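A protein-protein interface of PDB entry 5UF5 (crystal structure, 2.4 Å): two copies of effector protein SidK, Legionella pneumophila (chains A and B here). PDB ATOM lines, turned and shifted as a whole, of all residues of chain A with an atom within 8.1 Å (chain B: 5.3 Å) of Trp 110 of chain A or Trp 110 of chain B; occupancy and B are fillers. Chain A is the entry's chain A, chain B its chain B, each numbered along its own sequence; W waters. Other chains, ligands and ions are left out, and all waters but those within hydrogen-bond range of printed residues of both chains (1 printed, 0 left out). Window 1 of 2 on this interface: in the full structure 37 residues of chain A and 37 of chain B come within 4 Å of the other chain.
OH of Tyr 114 of chain A lies within hydrogen-bond range of OE2 of Glu 78 of chain B (2.8 Å). A ring nitrogen (ND1) of His 115 of chain A lies within hydrogen-bond range of the side-chain carboxylate (OE2) of Glu 78 of chain B (2.7 Å). OE2 of Glu 78 of chain A lies within hydrogen-bond range of OH of Tyr 114 of chain B (3.0 Å). A ring nitrogen (NE2) of His 106 of chain A sits close to the backbone carbonyl oxygen (O) of Leu 109 of chain B (3.5 Å). A ring nitrogen (ND1) of His 115 of chain B sits at hydrogen-bond distance from the side-chain carboxylate (OE2) of Glu 78 of chain A (2.7 Å). The backbone carbonyl oxygen of Trp 110 of chain B sits at hydrogen-bond distance from a ring nitrogen (NE2) of His 106 of chain A. The backbone carbonyl oxygen (O) of Trp 110 of chain A sits at hydrogen-bond distance from a ring nitrogen (NE2) of His 106 of chain B, at 2.9 Å.
The side-chain amino group of Lys 111 of chain B is in hydrogen-bond range of a ring nitrogen (NE2) of His 115 of chain B, at 2.9 Å. O of Leu 109 of chain A is in hydrogen-bond range of OG of Ser 112 of chain A, at 2.8 Å. The backbone carbonyl oxygen (O) of Leu 109 of chain B is in hydrogen-bond range of the side-chain hydroxyl (OG) of Ser 112 of chain B, at 2.6 Å. The side-chain carboxylate (OE1) of Glu 78 of chain A lies within salt-bridge range of the guanidinium group (NH1) of Arg 81 of chain A, 2.7 Å away.
Glu 78 of chain A touches Trp 110 of chain B (OE2 to CH2, 3.6 Å). His 115 of chain B touches Arg 81 of chain A. Met 103 of chain A touches Tyr 114 of chain B. Trp 110 of chain B touches Val 107 of chain A. Val 107 of chain A touches Tyr 114 of chain B. CD1 of Leu 109 of chain A touches CD2 of Leu 109 of chain B, 3.8 Å away. CE3 of Trp 110 of chain A touches CB of Trp 110 of chain B, 3.4 Å away. CB of Asp 113 of chain A touches CE1 of His 106 of chain B (3.9 Å). CE1 of Tyr 114 of chain A touches CD2 of His 106 of chain B (3.3 Å). Val 107 of chain B touches Tyr 114 of chain A.
Of the printed residues of chain B, Glu 78 of chain A touches Trp 110, Tyr 114 and His 115. Of the printed residues of chain B, Val 107 of chain A touches Trp 110 (3.9 Å) and Tyr 114 (3.7 Å). Of the printed residues of chain A, Glu 78 of chain B touches Trp 110 (3.7 Å), Tyr 114 (2.8 Å), His 115 (2.7 Å) and Leu 118 (3.3 Å). Of the printed residues of chain A, Trp 110 of chain B touches Glu 78 (3.6 Å), His 106 (2.9 Å), Val 107 (3.9 Å) and Trp 110 (3.4 Å). Printed residues of chain A within 4 Å of His 115 of chain B: Glu 78 (2.7 Å) and Arg 81 (3.9 Å). The nearest printed residue of chain A that does not touch His 106 of chain B is Lys 111 of chain A (4.9 Å).
Of the 11 printed residues of chain B, 8 touch a printed residue of chain A. Printed residues of chain B that touch a printed residue of chain A: Glu 78, His 106, Val 107, Leu 109, Trp 110, Ser 112, Tyr 114 and His 115. Among the printed residues, 25 pairs touch across the chains. Among the printed residues, no Asp or Glu carboxylate lies within 4 Å of a Lys or Arg side-chain nitrogen of the other chain.
Glu 78 of chain A touches Tyr 114 of chain B, and with the chains exchanged Tyr 114 of chain A touches Glu 78 of chain B. His 106 of chain A touches Leu 109 of chain B, and with the chains exchanged Leu 109 of chain A touches His 106 of chain B. His 106 of chain A touches Tyr 114 of chain B, and with the chains exchanged Tyr 114 of chain A touches His 106 of chain B. Val 107 of chain A touches Trp 110 of chain B, and with the chains exchanged Trp 110 of chain A touches Val 107 of chain B. Positions printed for both chains: 74, 78, 106, 107, 108, 109, 110, 111, 112, 114 and 115.
Water W1 bridges the backbone carbonyl oxygen of His 106 of chain B (3.0 Å) and the backbone NH of Trp 110 of chain A (3.4 Å).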
ATOM      1  N   ARG A  71     -27.028  34.997   3.333  1.00  0.00           N
ATOM      2  CA  ARG A  71     -27.328  33.587   3.095  1.00  0.00           C
ATOM      3  C   ARG A  71     -28.600  33.163   3.822  1.00  0.00           C
ATOM      4  O   ARG A  71     -29.490  32.545   3.225  1.00  0.00           O
ATOM      5  CB  ARG A  71     -26.146  32.723   3.533  1.00  0.00           C
ATOM      6  CG  ARG A  71     -26.433  31.230   3.532  1.00  0.00           C
ATOM      7  CD  ARG A  71     -25.247  30.436   4.074  1.00  0.00           C
ATOM      8  NE  ARG A  71     -24.864  30.881   5.410  1.00  0.00           N
ATOM      9  CZ  ARG A  71     -25.494  30.521   6.526  1.00  0.00           C
ATOM     10  NH1 ARG A  71     -26.542  29.707   6.464  1.00  0.00           N
ATOM     11  NH2 ARG A  71     -25.081  30.977   7.701  1.00  0.00           N
ATOM     12  N   LEU A  74     -31.683  34.489   2.117  1.00  0.00           N
ATOM     13  CA  LEU A  74     -32.049  33.827   0.869  1.00  0.00           C
ATOM     14  C   LEU A  74     -32.833  32.544   1.117  1.00  0.00           C
ATOM     15  O   LEU A  74     -33.732  32.207   0.338  1.00  0.00           O
ATOM     16  CB  LEU A  74     -30.798  33.531   0.038  1.00  0.00           C
ATOM     17  CG  LEU A  74     -31.050  32.896  -1.332  1.00  0.00           C
ATOM     18  CD1 LEU A  74     -31.995  33.758  -2.161  1.00  0.00           C
ATOM     19  CD2 LEU A  74     -29.740  32.655  -2.080  1.00  0.00           C
ATOM     20  N   ILE A  75     -32.517  31.825   2.196  1.00  0.00           N
ATOM     21  CA  ILE A  75     -33.287  30.634   2.548  1.00  0.00           C
ATOM     22  C   ILE A  75     -34.759  30.992   2.739  1.00  0.00           C
ATOM     23  O   ILE A  75     -35.649  30.372   2.145  1.00  0.00           O
ATOM     24  CB  ILE A  75     -32.696  29.966   3.802  1.00  0.00           C
ATOM     25  CG1 ILE A  75     -31.244  29.555   3.545  1.00  0.00           C
ATOM     26  CG2 ILE A  75     -33.535  28.766   4.208  1.00  0.00           C
ATOM     27  CD1 ILE A  75     -30.522  29.040   4.765  1.00  0.00           C
ATOM     28  N   GLN A  77     -36.249  33.723   1.731  1.00  0.00           N
ATOM     29  CA  GLN A  77     -36.773  34.267   0.481  1.00  0.00           C
ATOM     30  C   GLN A  77     -37.262  33.154  -0.438  1.00  0.00           C
ATOM     31  O   GLN A  77     -38.327  33.269  -1.056  1.00  0.00           O
ATOM     32  CB  GLN A  77     -35.700  35.104  -0.213  1.00  0.00           C
ATOM     33  CG  GLN A  77     -36.139  35.705  -1.536  1.00  0.00           C
ATOM     34  CD  GLN A  77     -35.029  36.475  -2.222  1.00  0.00           C
ATOM     35  OE1 GLN A  77     -34.322  37.261  -1.592  1.00  0.00           O
ATOM     36  NE2 GLN A  77     -34.864  36.246  -3.519  1.00  0.00           N
ATOM     37  N   GLU A  78     -36.495  32.064  -0.536  1.00  0.00           N
ATOM     38  CA  GLU A  78     -36.923  30.915  -1.328  1.00  0.00           C
ATOM     39  C   GLU A  78     -38.161  30.258  -0.728  1.00  0.00           C
ATOM     40  O   GLU A  78     -39.106  29.922  -1.451  1.00  0.00           O
ATOM     41  CB  GLU A  78     -35.779  29.905  -1.436  1.00  0.00           C
ATOM     42  CG  GLU A  78     -34.592  30.365  -2.276  1.00  0.00           C
ATOM     43  CD  GLU A  78     -34.845  30.230  -3.768  1.00  0.00           C
ATOM     44  OE1 GLU A  78     -35.485  31.129  -4.353  1.00  0.00           O
ATOM     45  OE2 GLU A  78     -34.413  29.213  -4.351  1.00  0.00           O
ATOM     46  N   ARG A  81     -41.102  32.255  -1.508  1.00  0.00           N
ATOM     47  CA  ARG A  81     -41.491  32.081  -2.906  1.00  0.00           C
ATOM     48  C   ARG A  81     -42.393  30.867  -3.084  1.00  0.00           C
ATOM     49  O   ARG A  81     -43.393  30.932  -3.805  1.00  0.00           O
ATOM     50  CB  ARG A  81     -40.255  31.940  -3.795  1.00  0.00           C
ATOM     51  CG  ARG A  81     -39.687  33.236  -4.329  1.00  0.00           C
ATOM     52  CD  ARG A  81     -38.472  32.954  -5.200  1.00  0.00           C
ATOM     53  NE  ARG A  81     -38.835  32.347  -6.476  1.00  0.00           N
ATOM     54  CZ  ARG A  81     -38.050  31.517  -7.158  1.00  0.00           C
ATOM     55  NH1 ARG A  81     -36.863  31.177  -6.676  1.00  0.00           N
ATOM     56  NH2 ARG A  81     -38.458  31.017  -8.316  1.00  0.00           N
ATOM     57  N   MET A 103     -34.200  23.349   1.438  1.00  0.00           N
ATOM     58  CA  MET A 103     -33.809  24.641   0.883  1.00  0.00           C
ATOM     59  C   MET A 103     -32.585  25.198   1.596  1.00  0.00           C
ATOM     60  O   MET A 103     -31.702  25.788   0.961  1.00  0.00           O
ATOM     61  CB  MET A 103     -34.971  25.631   0.971  1.00  0.00           C
ATOM     62  CG  MET A 103     -36.124  25.335   0.032  1.00  0.00           C
ATOM     63  SD  MET A 103     -37.409  26.600   0.111  1.00  0.00           S
ATOM     64  CE  MET A 103     -38.595  25.960  -1.069  1.00  0.00           C
ATOM     65  N   LYS A 104     -32.514  25.017   2.918  1.00  0.00           N
ATOM     66  CA  LYS A 104     -31.376  25.515   3.683  1.00  0.00           C
ATOM     67  C   LYS A 104     -30.071  24.901   3.192  1.00  0.00           C
ATOM     68  O   LYS A 104     -29.078  25.607   2.986  1.00  0.00           O
ATOM     69  CB  LYS A 104     -31.577  25.230   5.173  1.00  0.00           C
ATOM     70  CG  LYS A 104     -30.295  25.313   5.989  1.00  0.00           C
ATOM     71  CD  LYS A 104     -30.572  25.361   7.483  1.00  0.00           C
ATOM     72  CE  LYS A 104     -31.361  24.154   7.941  1.00  0.00           C
ATOM     73  NZ  LYS A 104     -31.555  24.158   9.417  1.00  0.00           N
ATOM     74  N   GLN A 105     -30.056  23.583   2.997  1.00  0.00           N
ATOM     75  CA  GLN A 105     -28.835  22.931   2.538  1.00  0.00           C
ATOM     76  C   GLN A 105     -28.496  23.318   1.104  1.00  0.00           C
ATOM     77  O   GLN A 105     -27.315  23.398   0.750  1.00  0.00           O
ATOM     78  CB  GLN A 105     -28.970  21.413   2.667  1.00  0.00           C
ATOM     79  CG  GLN A 105     -29.328  20.941   4.073  1.00  0.00           C
ATOM     80  CD  GLN A 105     -28.326  21.393   5.125  1.00  0.00           C
ATOM     81  OE1 GLN A 105     -27.132  21.534   4.848  1.00  0.00           O
ATOM     82  NE2 GLN A 105     -28.811  21.624   6.341  1.00  0.00           N
ATOM     83  N   HIS A 106     -29.509  23.570   0.274  1.00  0.00           N
ATOM     84  CA  HIS A 106     -29.253  23.947  -1.112  1.00  0.00           C
ATOM     85  C   HIS A 106     -28.667  25.352  -1.196  1.00  0.00           C
ATOM     86  O   HIS A 106     -27.682  25.584  -1.909  1.00  0.00           O
ATOM     87  CB  HIS A 106     -30.547  23.848  -1.920  1.00  0.00           C
ATOM     88  CG  HIS A 106     -30.344  23.927  -3.400  1.00  0.00           C
ATOM     89  ND1 HIS A 106     -29.743  22.919  -4.124  1.00  0.00           N
ATOM     90  CD2 HIS A 106     -30.662  24.893  -4.294  1.00  0.00           C
ATOM     91  CE1 HIS A 106     -29.702  23.260  -5.398  1.00  0.00           C
ATOM     92  NE2 HIS A 106     -30.250  24.454  -5.529  1.00  0.00           N
ATOM     93  N   VAL A 107     -29.256  26.300  -0.465  1.00  0.00           N
ATOM     94  CA  VAL A 107     -28.747  27.668  -0.460  1.00  0.00           C
ATOM     95  C   VAL A 107     -27.355  27.721   0.159  1.00  0.00           C
ATOM     96  O   VAL A 107     -26.483  28.465  -0.306  1.00  0.00           O
ATOM     97  CB  VAL A 107     -29.735  28.596   0.270  1.00  0.00           C
ATOM     98  CG1 VAL A 107     -29.133  29.978   0.477  1.00  0.00           C
ATOM     99  CG2 VAL A 107     -31.034  28.694  -0.509  1.00  0.00           C
ATOM    100  N   ASN A 108     -27.116  26.923   1.203  1.00  0.00           N
ATOM    101  CA  ASN A 108     -25.803  26.920   1.841  1.00  0.00           C
ATOM    102  C   ASN A 108     -24.712  26.449   0.889  1.00  0.00           C
ATOM    103  O   ASN A 108     -23.559  26.879   1.007  1.00  0.00           O
ATOM    104  CB  ASN A 108     -25.827  26.052   3.097  1.00  0.00           C
ATOM    105  CG  ASN A 108     -26.554  26.719   4.247  1.00  0.00           C
ATOM    106  OD1 ASN A 108     -27.153  27.781   4.084  1.00  0.00           O
ATOM    107  ND2 ASN A 108     -26.511  26.095   5.418  1.00  0.00           N
ATOM    108  N   LEU A 109     -25.048  25.567  -0.056  1.00  0.00           N
ATOM    109  CA  LEU A 109     -24.082  25.191  -1.084  1.00  0.00           C
ATOM    110  C   LEU A 109     -23.826  26.346  -2.044  1.00  0.00           C
ATOM    111  O   LEU A 109     -22.683  26.585  -2.446  1.00  0.00           O
ATOM    112  CB  LEU A 109     -24.575  23.959  -1.844  1.00  0.00           C
ATOM    113  CG  LEU A 109     -24.517  22.617  -1.111  1.00  0.00           C
ATOM    114  CD1 LEU A 109     -25.255  21.548  -1.901  1.00  0.00           C
ATOM    115  CD2 LEU A 109     -23.071  22.202  -0.868  1.00  0.00           C
ATOM    116  N   TRP A 110     -24.879  27.077  -2.411  1.00  0.00           N
ATOM    117  CA  TRP A 110     -24.733  28.208  -3.321  1.00  0.00           C
ATOM    118  C   TRP A 110     -23.943  29.338  -2.670  1.00  0.00           C
ATOM    119  O   TRP A 110     -22.955  29.824  -3.237  1.00  0.00           O
ATOM    120  CB  TRP A 110     -26.121  28.679  -3.765  1.00  0.00           C
ATOM    121  CG  TRP A 110     -26.162  29.960  -4.555  1.00  0.00           C
ATOM    122  CD1 TRP A 110     -26.848  31.095  -4.229  1.00  0.00           C
ATOM    123  CD2 TRP A 110     -25.511  30.229  -5.807  1.00  0.00           C
ATOM    124  NE1 TRP A 110     -26.658  32.054  -5.194  1.00  0.00           N
ATOM    125  CE2 TRP A 110     -25.844  31.549  -6.173  1.00  0.00           C
ATOM    126  CE3 TRP A 110     -24.677  29.487  -6.648  1.00  0.00           C
ATOM    127  CZ2 TRP A 110     -25.374  32.141  -7.345  1.00  0.00           C
ATOM    128  CZ3 TRP A 110     -24.210  30.076  -7.813  1.00  0.00           C
ATOM    129  CH2 TRP A 110     -24.559  31.392  -8.149  1.00  0.00           C
ATOM    130  N   LYS A 111     -24.349  29.754  -1.470  1.00  0.00           N
ATOM    131  CA  LYS A 111     -23.691  30.841  -0.744  1.00  0.00           C
ATOM    132  C   LYS A 111     -22.470  30.293   0.001  1.00  0.00           C
ATOM    133  O   LYS A 111     -22.422  30.206   1.231  1.00  0.00           O
ATOM    134  CB  LYS A 111     -24.667  31.514   0.209  1.00  0.00           C
ATOM    135  CG  LYS A 111     -25.794  32.264  -0.482  1.00  0.00           C
ATOM    136  CD  LYS A 111     -25.264  33.455  -1.264  1.00  0.00           C
ATOM    137  CE  LYS A 111     -26.387  34.178  -1.990  1.00  0.00           C
ATOM    138  NZ  LYS A 111     -25.875  35.271  -2.856  1.00  0.00           N
ATOM    139  N   SER A 112     -21.463  29.927  -0.784  1.00  0.00           N
ATOM    140  CA  SER A 112     -20.206  29.405  -0.263  1.00  0.00           C
ATOM    141  C   SER A 112     -19.180  29.448  -1.389  1.00  0.00           C
ATOM    142  O   SER A 112     -19.483  29.862  -2.511  1.00  0.00           O
ATOM    143  CB  SER A 112     -20.377  27.984   0.283  1.00  0.00           C
ATOM    144  OG  SER A 112     -20.511  27.054  -0.780  1.00  0.00           O
ATOM    145  N   ASP A 113     -17.958  29.037  -1.067  1.00  0.00           N
ATOM    146  CA  ASP A 113     -16.881  28.811  -2.043  1.00  0.00           C
ATOM    147  C   ASP A 113     -16.524  30.141  -2.712  1.00  0.00           C
ATOM    148  O   ASP A 113     -16.491  31.182  -2.039  1.00  0.00           O
ATOM    149  CB  ASP A 113     -17.297  27.728  -3.007  1.00  0.00           C
ATOM    150  CG  ASP A 113     -16.116  26.999  -3.594  1.00  0.00           C
ATOM    151  OD1 ASP A 113     -15.559  27.470  -4.610  1.00  0.00           O
ATOM    152  OD2 ASP A 113     -15.751  25.946  -3.032  1.00  0.00           O
ATOM    153  N   TYR A 114     -16.252  30.129  -4.021  1.00  0.00           N
ATOM    154  CA  TYR A 114     -15.867  31.344  -4.732  1.00  0.00           C
ATOM    155  C   TYR A 114     -16.954  32.409  -4.655  1.00  0.00           C
ATOM    156  O   TYR A 114     -16.652  33.606  -4.706  1.00  0.00           O
ATOM    157  CB  TYR A 114     -15.571  31.021  -6.201  1.00  0.00           C
ATOM    158  CG  TYR A 114     -16.827  31.030  -7.051  1.00  0.00           C
ATOM    159  CD1 TYR A 114     -17.615  29.895  -7.177  1.00  0.00           C
ATOM    160  CD2 TYR A 114     -17.246  32.189  -7.696  1.00  0.00           C
ATOM    161  CE1 TYR A 114     -18.776  29.910  -7.929  1.00  0.00           C
ATOM    162  CE2 TYR A 114     -18.405  32.214  -8.440  1.00  0.00           C
ATOM    163  CZ  TYR A 114     -19.165  31.072  -8.555  1.00  0.00           C
ATOM    164  OH  TYR A 114     -20.317  31.097  -9.306  1.00  0.00           O
ATOM    165  N   HIS A 115     -18.221  31.992  -4.572  1.00  0.00           N
ATOM    166  CA  HIS A 115     -19.327  32.936  -4.696  1.00  0.00           C
ATOM    167  C   HIS A 115     -19.319  33.954  -3.562  1.00  0.00           C
ATOM    168  O   HIS A 115     -19.603  35.137  -3.779  1.00  0.00           O
ATOM    169  CB  HIS A 115     -20.658  32.183  -4.735  1.00  0.00           C
ATOM    170  CG  HIS A 115     -21.856  33.076  -4.835  1.00  0.00           C
ATOM    171  ND1 HIS A 115     -22.277  33.623  -6.027  1.00  0.00           N
ATOM    172  CD2 HIS A 115     -22.721  33.516  -3.892  1.00  0.00           C
ATOM    173  CE1 HIS A 115     -23.351  34.364  -5.814  1.00  0.00           C
ATOM    174  NE2 HIS A 115     -23.641  34.316  -4.526  1.00  0.00           N
ATOM    175  N   VAL A 116     -19.003  33.511  -2.342  1.00  0.00           N
ATOM    176  CA  VAL A 116     -18.941  34.435  -1.214  1.00  0.00           C
ATOM    177  C   VAL A 116     -17.799  35.425  -1.392  1.00  0.00           C
ATOM    178  O   VAL A 116     -17.964  36.631  -1.164  1.00  0.00           O
ATOM    179  CB  VAL A 116     -18.810  33.657   0.107  1.00  0.00           C
ATOM    180  CG1 VAL A 116     -18.472  34.609   1.245  1.00  0.00           C
ATOM    181  CG2 VAL A 116     -20.094  32.906   0.402  1.00  0.00           C
ATOM    182  N   LEU A 118     -16.499  36.379  -4.177  1.00  0.00           N
ATOM    183  CA  LEU A 118     -16.891  37.293  -5.243  1.00  0.00           C
ATOM    184  C   LEU A 118     -17.835  38.369  -4.720  1.00  0.00           C
ATOM    185  O   LEU A 118     -17.729  39.538  -5.109  1.00  0.00           O
ATOM    186  CB  LEU A 118     -17.537  36.516  -6.390  1.00  0.00           C
ATOM    187  CG  LEU A 118     -17.787  37.309  -7.674  1.00  0.00           C
ATOM    188  CD1 LEU A 118     -16.530  38.052  -8.095  1.00  0.00           C
ATOM    189  CD2 LEU A 118     -18.264  36.390  -8.787  1.00  0.00           C
ATOM    190  N   ASN A 119     -18.756  37.994  -3.825  1.00  0.00           N
ATOM    191  CA  ASN A 119     -19.648  38.980  -3.222  1.00  0.00           C
ATOM    192  C   ASN A 119     -18.875  39.970  -2.359  1.00  0.00           C
ATOM    193  O   ASN A 119     -19.182  41.169  -2.353  1.00  0.00           O
ATOM    194  CB  ASN A 119     -20.728  38.279  -2.394  1.00  0.00           C
ATOM    195  CG  ASN A 119     -21.697  37.482  -3.249  1.00  0.00           C
ATOM    196  OD1 ASN A 119     -21.951  37.820  -4.405  1.00  0.00           O
ATOM    197  ND2 ASN A 119     -22.250  36.421  -2.676  1.00  0.00           N
ATOM    198  N   LEU B  74     -26.206  32.796 -16.014  1.00  0.00           N
ATOM    199  CA  LEU B  74     -25.680  33.047 -14.676  1.00  0.00           C
ATOM    200  C   LEU B  74     -24.207  32.678 -14.581  1.00  0.00           C
ATOM    201  O   LEU B  74     -23.445  33.350 -13.876  1.00  0.00           O
ATOM    202  CB  LEU B  74     -26.500  32.283 -13.633  1.00  0.00           C
ATOM    203  CG  LEU B  74     -26.096  32.471 -12.167  1.00  0.00           C
ATOM    204  CD1 LEU B  74     -25.973  33.948 -11.822  1.00  0.00           C
ATOM    205  CD2 LEU B  74     -27.087  31.785 -11.236  1.00  0.00           C
ATOM    206  N   GLU B  78     -21.458  35.437 -13.456  1.00  0.00           N
ATOM    207  CA  GLU B  78     -20.520  35.269 -12.350  1.00  0.00           C
ATOM    208  C   GLU B  78     -19.094  35.561 -12.799  1.00  0.00           C
ATOM    209  O   GLU B  78     -18.343  36.262 -12.109  1.00  0.00           O
ATOM    210  CB  GLU B  78     -20.621  33.849 -11.786  1.00  0.00           C
ATOM    211  CG  GLU B  78     -21.910  33.543 -11.032  1.00  0.00           C
ATOM    212  CD  GLU B  78     -21.945  34.170  -9.648  1.00  0.00           C
ATOM    213  OE1 GLU B  78     -22.333  35.353  -9.533  1.00  0.00           O
ATOM    214  OE2 GLU B  78     -21.570  33.481  -8.675  1.00  0.00           O
ATOM    215  N   HIS B 106     -20.518  25.038 -10.024  1.00  0.00           N
ATOM    216  CA  HIS B 106     -21.148  25.648  -8.857  1.00  0.00           C
ATOM    217  C   HIS B 106     -22.541  26.168  -9.197  1.00  0.00           C
ATOM    218  O   HIS B 106     -23.503  25.929  -8.458  1.00  0.00           O
ATOM    219  CB  HIS B 106     -20.263  26.772  -8.320  1.00  0.00           C
ATOM    220  CG  HIS B 106     -20.676  27.280  -6.974  1.00  0.00           C
ATOM    221  ND1 HIS B 106     -20.301  26.662  -5.799  1.00  0.00           N
ATOM    222  CD2 HIS B 106     -21.425  28.349  -6.614  1.00  0.00           C
ATOM    223  CE1 HIS B 106     -20.806  27.326  -4.774  1.00  0.00           C
ATOM    224  NE2 HIS B 106     -21.492  28.353  -5.242  1.00  0.00           N
ATOM    225  N   VAL B 107     -22.667  26.875 -10.322  1.00  0.00           N
ATOM    226  CA  VAL B 107     -23.961  27.405 -10.741  1.00  0.00           C
ATOM    227  C   VAL B 107     -24.907  26.275 -11.129  1.00  0.00           C
ATOM    228  O   VAL B 107     -26.105  26.320 -10.823  1.00  0.00           O
ATOM    229  CB  VAL B 107     -23.771  28.409 -11.892  1.00  0.00           C
ATOM    230  CG1 VAL B 107     -25.107  28.749 -12.536  1.00  0.00           C
ATOM    231  CG2 VAL B 107     -23.081  29.668 -11.387  1.00  0.00           C
ATOM    232  N   ASN B 108     -24.387  25.245 -11.807  1.00  0.00           N
ATOM    233  CA  ASN B 108     -25.236  24.135 -12.237  1.00  0.00           C
ATOM    234  C   ASN B 108     -25.904  23.454 -11.051  1.00  0.00           C
ATOM    235  O   ASN B 108     -27.062  23.030 -11.143  1.00  0.00           O
ATOM    236  CB  ASN B 108     -24.421  23.119 -13.039  1.00  0.00           C
ATOM    237  CG  ASN B 108     -24.087  23.608 -14.437  1.00  0.00           C
ATOM    238  OD1 ASN B 108     -24.621  24.614 -14.902  1.00  0.00           O
ATOM    239  ND2 ASN B 108     -23.206  22.882 -15.119  1.00  0.00           N
ATOM    240  N   LEU B 109     -25.191  23.335  -9.927  1.00  0.00           N
ATOM    241  CA  LEU B 109     -25.789  22.728  -8.742  1.00  0.00           C
ATOM    242  C   LEU B 109     -26.878  23.620  -8.162  1.00  0.00           C
ATOM    243  O   LEU B 109     -27.930  23.128  -7.736  1.00  0.00           O
ATOM    244  CB  LEU B 109     -24.707  22.439  -7.699  1.00  0.00           C
ATOM    245  CG  LEU B 109     -25.173  21.891  -6.348  1.00  0.00           C
ATOM    246  CD1 LEU B 109     -26.073  20.675  -6.525  1.00  0.00           C
ATOM    247  CD2 LEU B 109     -23.978  21.550  -5.468  1.00  0.00           C
ATOM    248  N   TRP B 110     -26.645  24.933  -8.148  1.00  0.00           N
ATOM    249  CA  TRP B 110     -27.648  25.875  -7.665  1.00  0.00           C
ATOM    250  C   TRP B 110     -28.877  25.879  -8.563  1.00  0.00           C
ATOM    251  O   TRP B 110     -30.012  25.862  -8.072  1.00  0.00           O
ATOM    252  CB  TRP B 110     -27.025  27.270  -7.574  1.00  0.00           C
ATOM    253  CG  TRP B 110     -27.982  28.413  -7.397  1.00  0.00           C
ATOM    254  CD1 TRP B 110     -28.149  29.477  -8.237  1.00  0.00           C
ATOM    255  CD2 TRP B 110     -28.889  28.620  -6.305  1.00  0.00           C
ATOM    256  NE1 TRP B 110     -29.107  30.329  -7.742  1.00  0.00           N
ATOM    257  CE2 TRP B 110     -29.576  29.826  -6.556  1.00  0.00           C
ATOM    258  CE3 TRP B 110     -29.187  27.904  -5.142  1.00  0.00           C
ATOM    259  CZ2 TRP B 110     -30.543  30.330  -5.687  1.00  0.00           C
ATOM    260  CZ3 TRP B 110     -30.148  28.404  -4.281  1.00  0.00           C
ATOM    261  CH2 TRP B 110     -30.815  29.606  -4.559  1.00  0.00           C
ATOM    262  N   LYS B 111     -28.673  25.885  -9.880  1.00  0.00           N
ATOM    263  CA  LYS B 111     -29.774  25.856 -10.843  1.00  0.00           C
ATOM    264  C   LYS B 111     -30.201  24.407 -11.093  1.00  0.00           C
ATOM    265  O   LYS B 111     -30.060  23.851 -12.183  1.00  0.00           O
ATOM    266  CB  LYS B 111     -29.370  26.555 -12.135  1.00  0.00           C
ATOM    267  CG  LYS B 111     -29.222  28.064 -12.002  1.00  0.00           C
ATOM    268  CD  LYS B 111     -30.521  28.704 -11.533  1.00  0.00           C
ATOM    269  CE  LYS B 111     -30.390  30.215 -11.437  1.00  0.00           C
ATOM    270  NZ  LYS B 111     -31.657  30.861 -10.987  1.00  0.00           N
ATOM    271  N   SER B 112     -30.737  23.799 -10.040  1.00  0.00           N
ATOM    272  CA  SER B 112     -31.289  22.452 -10.111  1.00  0.00           C
ATOM    273  C   SER B 112     -32.206  22.251  -8.912  1.00  0.00           C
ATOM    274  O   SER B 112     -32.460  23.178  -8.138  1.00  0.00           O
ATOM    275  CB  SER B 112     -30.184  21.393 -10.145  1.00  0.00           C
ATOM    276  OG  SER B 112     -29.438  21.397  -8.941  1.00  0.00           O
ATOM    277  N   TYR B 114     -35.135  21.758  -6.238  1.00  0.00           N
ATOM    278  CA  TYR B 114     -36.375  22.508  -6.058  1.00  0.00           C
ATOM    279  C   TYR B 114     -36.311  23.874  -6.729  1.00  0.00           C
ATOM    280  O   TYR B 114     -37.350  24.433  -7.100  1.00  0.00           O
ATOM    281  CB  TYR B 114     -36.662  22.695  -4.568  1.00  0.00           C
ATOM    282  CG  TYR B 114     -35.859  23.838  -3.988  1.00  0.00           C
ATOM    283  CD1 TYR B 114     -34.541  23.653  -3.600  1.00  0.00           C
ATOM    284  CD2 TYR B 114     -36.407  25.113  -3.868  1.00  0.00           C
ATOM    285  CE1 TYR B 114     -33.795  24.698  -3.093  1.00  0.00           C
ATOM    286  CE2 TYR B 114     -35.666  26.163  -3.367  1.00  0.00           C
ATOM    287  CZ  TYR B 114     -34.362  25.950  -2.978  1.00  0.00           C
ATOM    288  OH  TYR B 114     -33.622  26.993  -2.473  1.00  0.00           O
ATOM    289  N   HIS B 115     -35.108  24.439  -6.861  1.00  0.00           N
ATOM    290  CA  HIS B 115     -34.978  25.825  -7.296  1.00  0.00           C
ATOM    291  C   HIS B 115     -35.507  26.021  -8.711  1.00  0.00           C
ATOM    292  O   HIS B 115     -36.223  26.992  -8.985  1.00  0.00           O
ATOM    293  CB  HIS B 115     -33.518  26.266  -7.206  1.00  0.00           C
ATOM    294  CG  HIS B 115     -33.292  27.677  -7.645  1.00  0.00           C
ATOM    295  ND1 HIS B 115     -33.611  28.761  -6.857  1.00  0.00           N
ATOM    296  CD2 HIS B 115     -32.792  28.183  -8.797  1.00  0.00           C
ATOM    297  CE1 HIS B 115     -33.311  29.874  -7.501  1.00  0.00           C
ATOM    298  NE2 HIS B 115     -32.812  29.550  -8.681  1.00  0.00           N
HETATM  299  O   HOH W   1     -24.148  25.888  -5.551  1.00  0.00           O
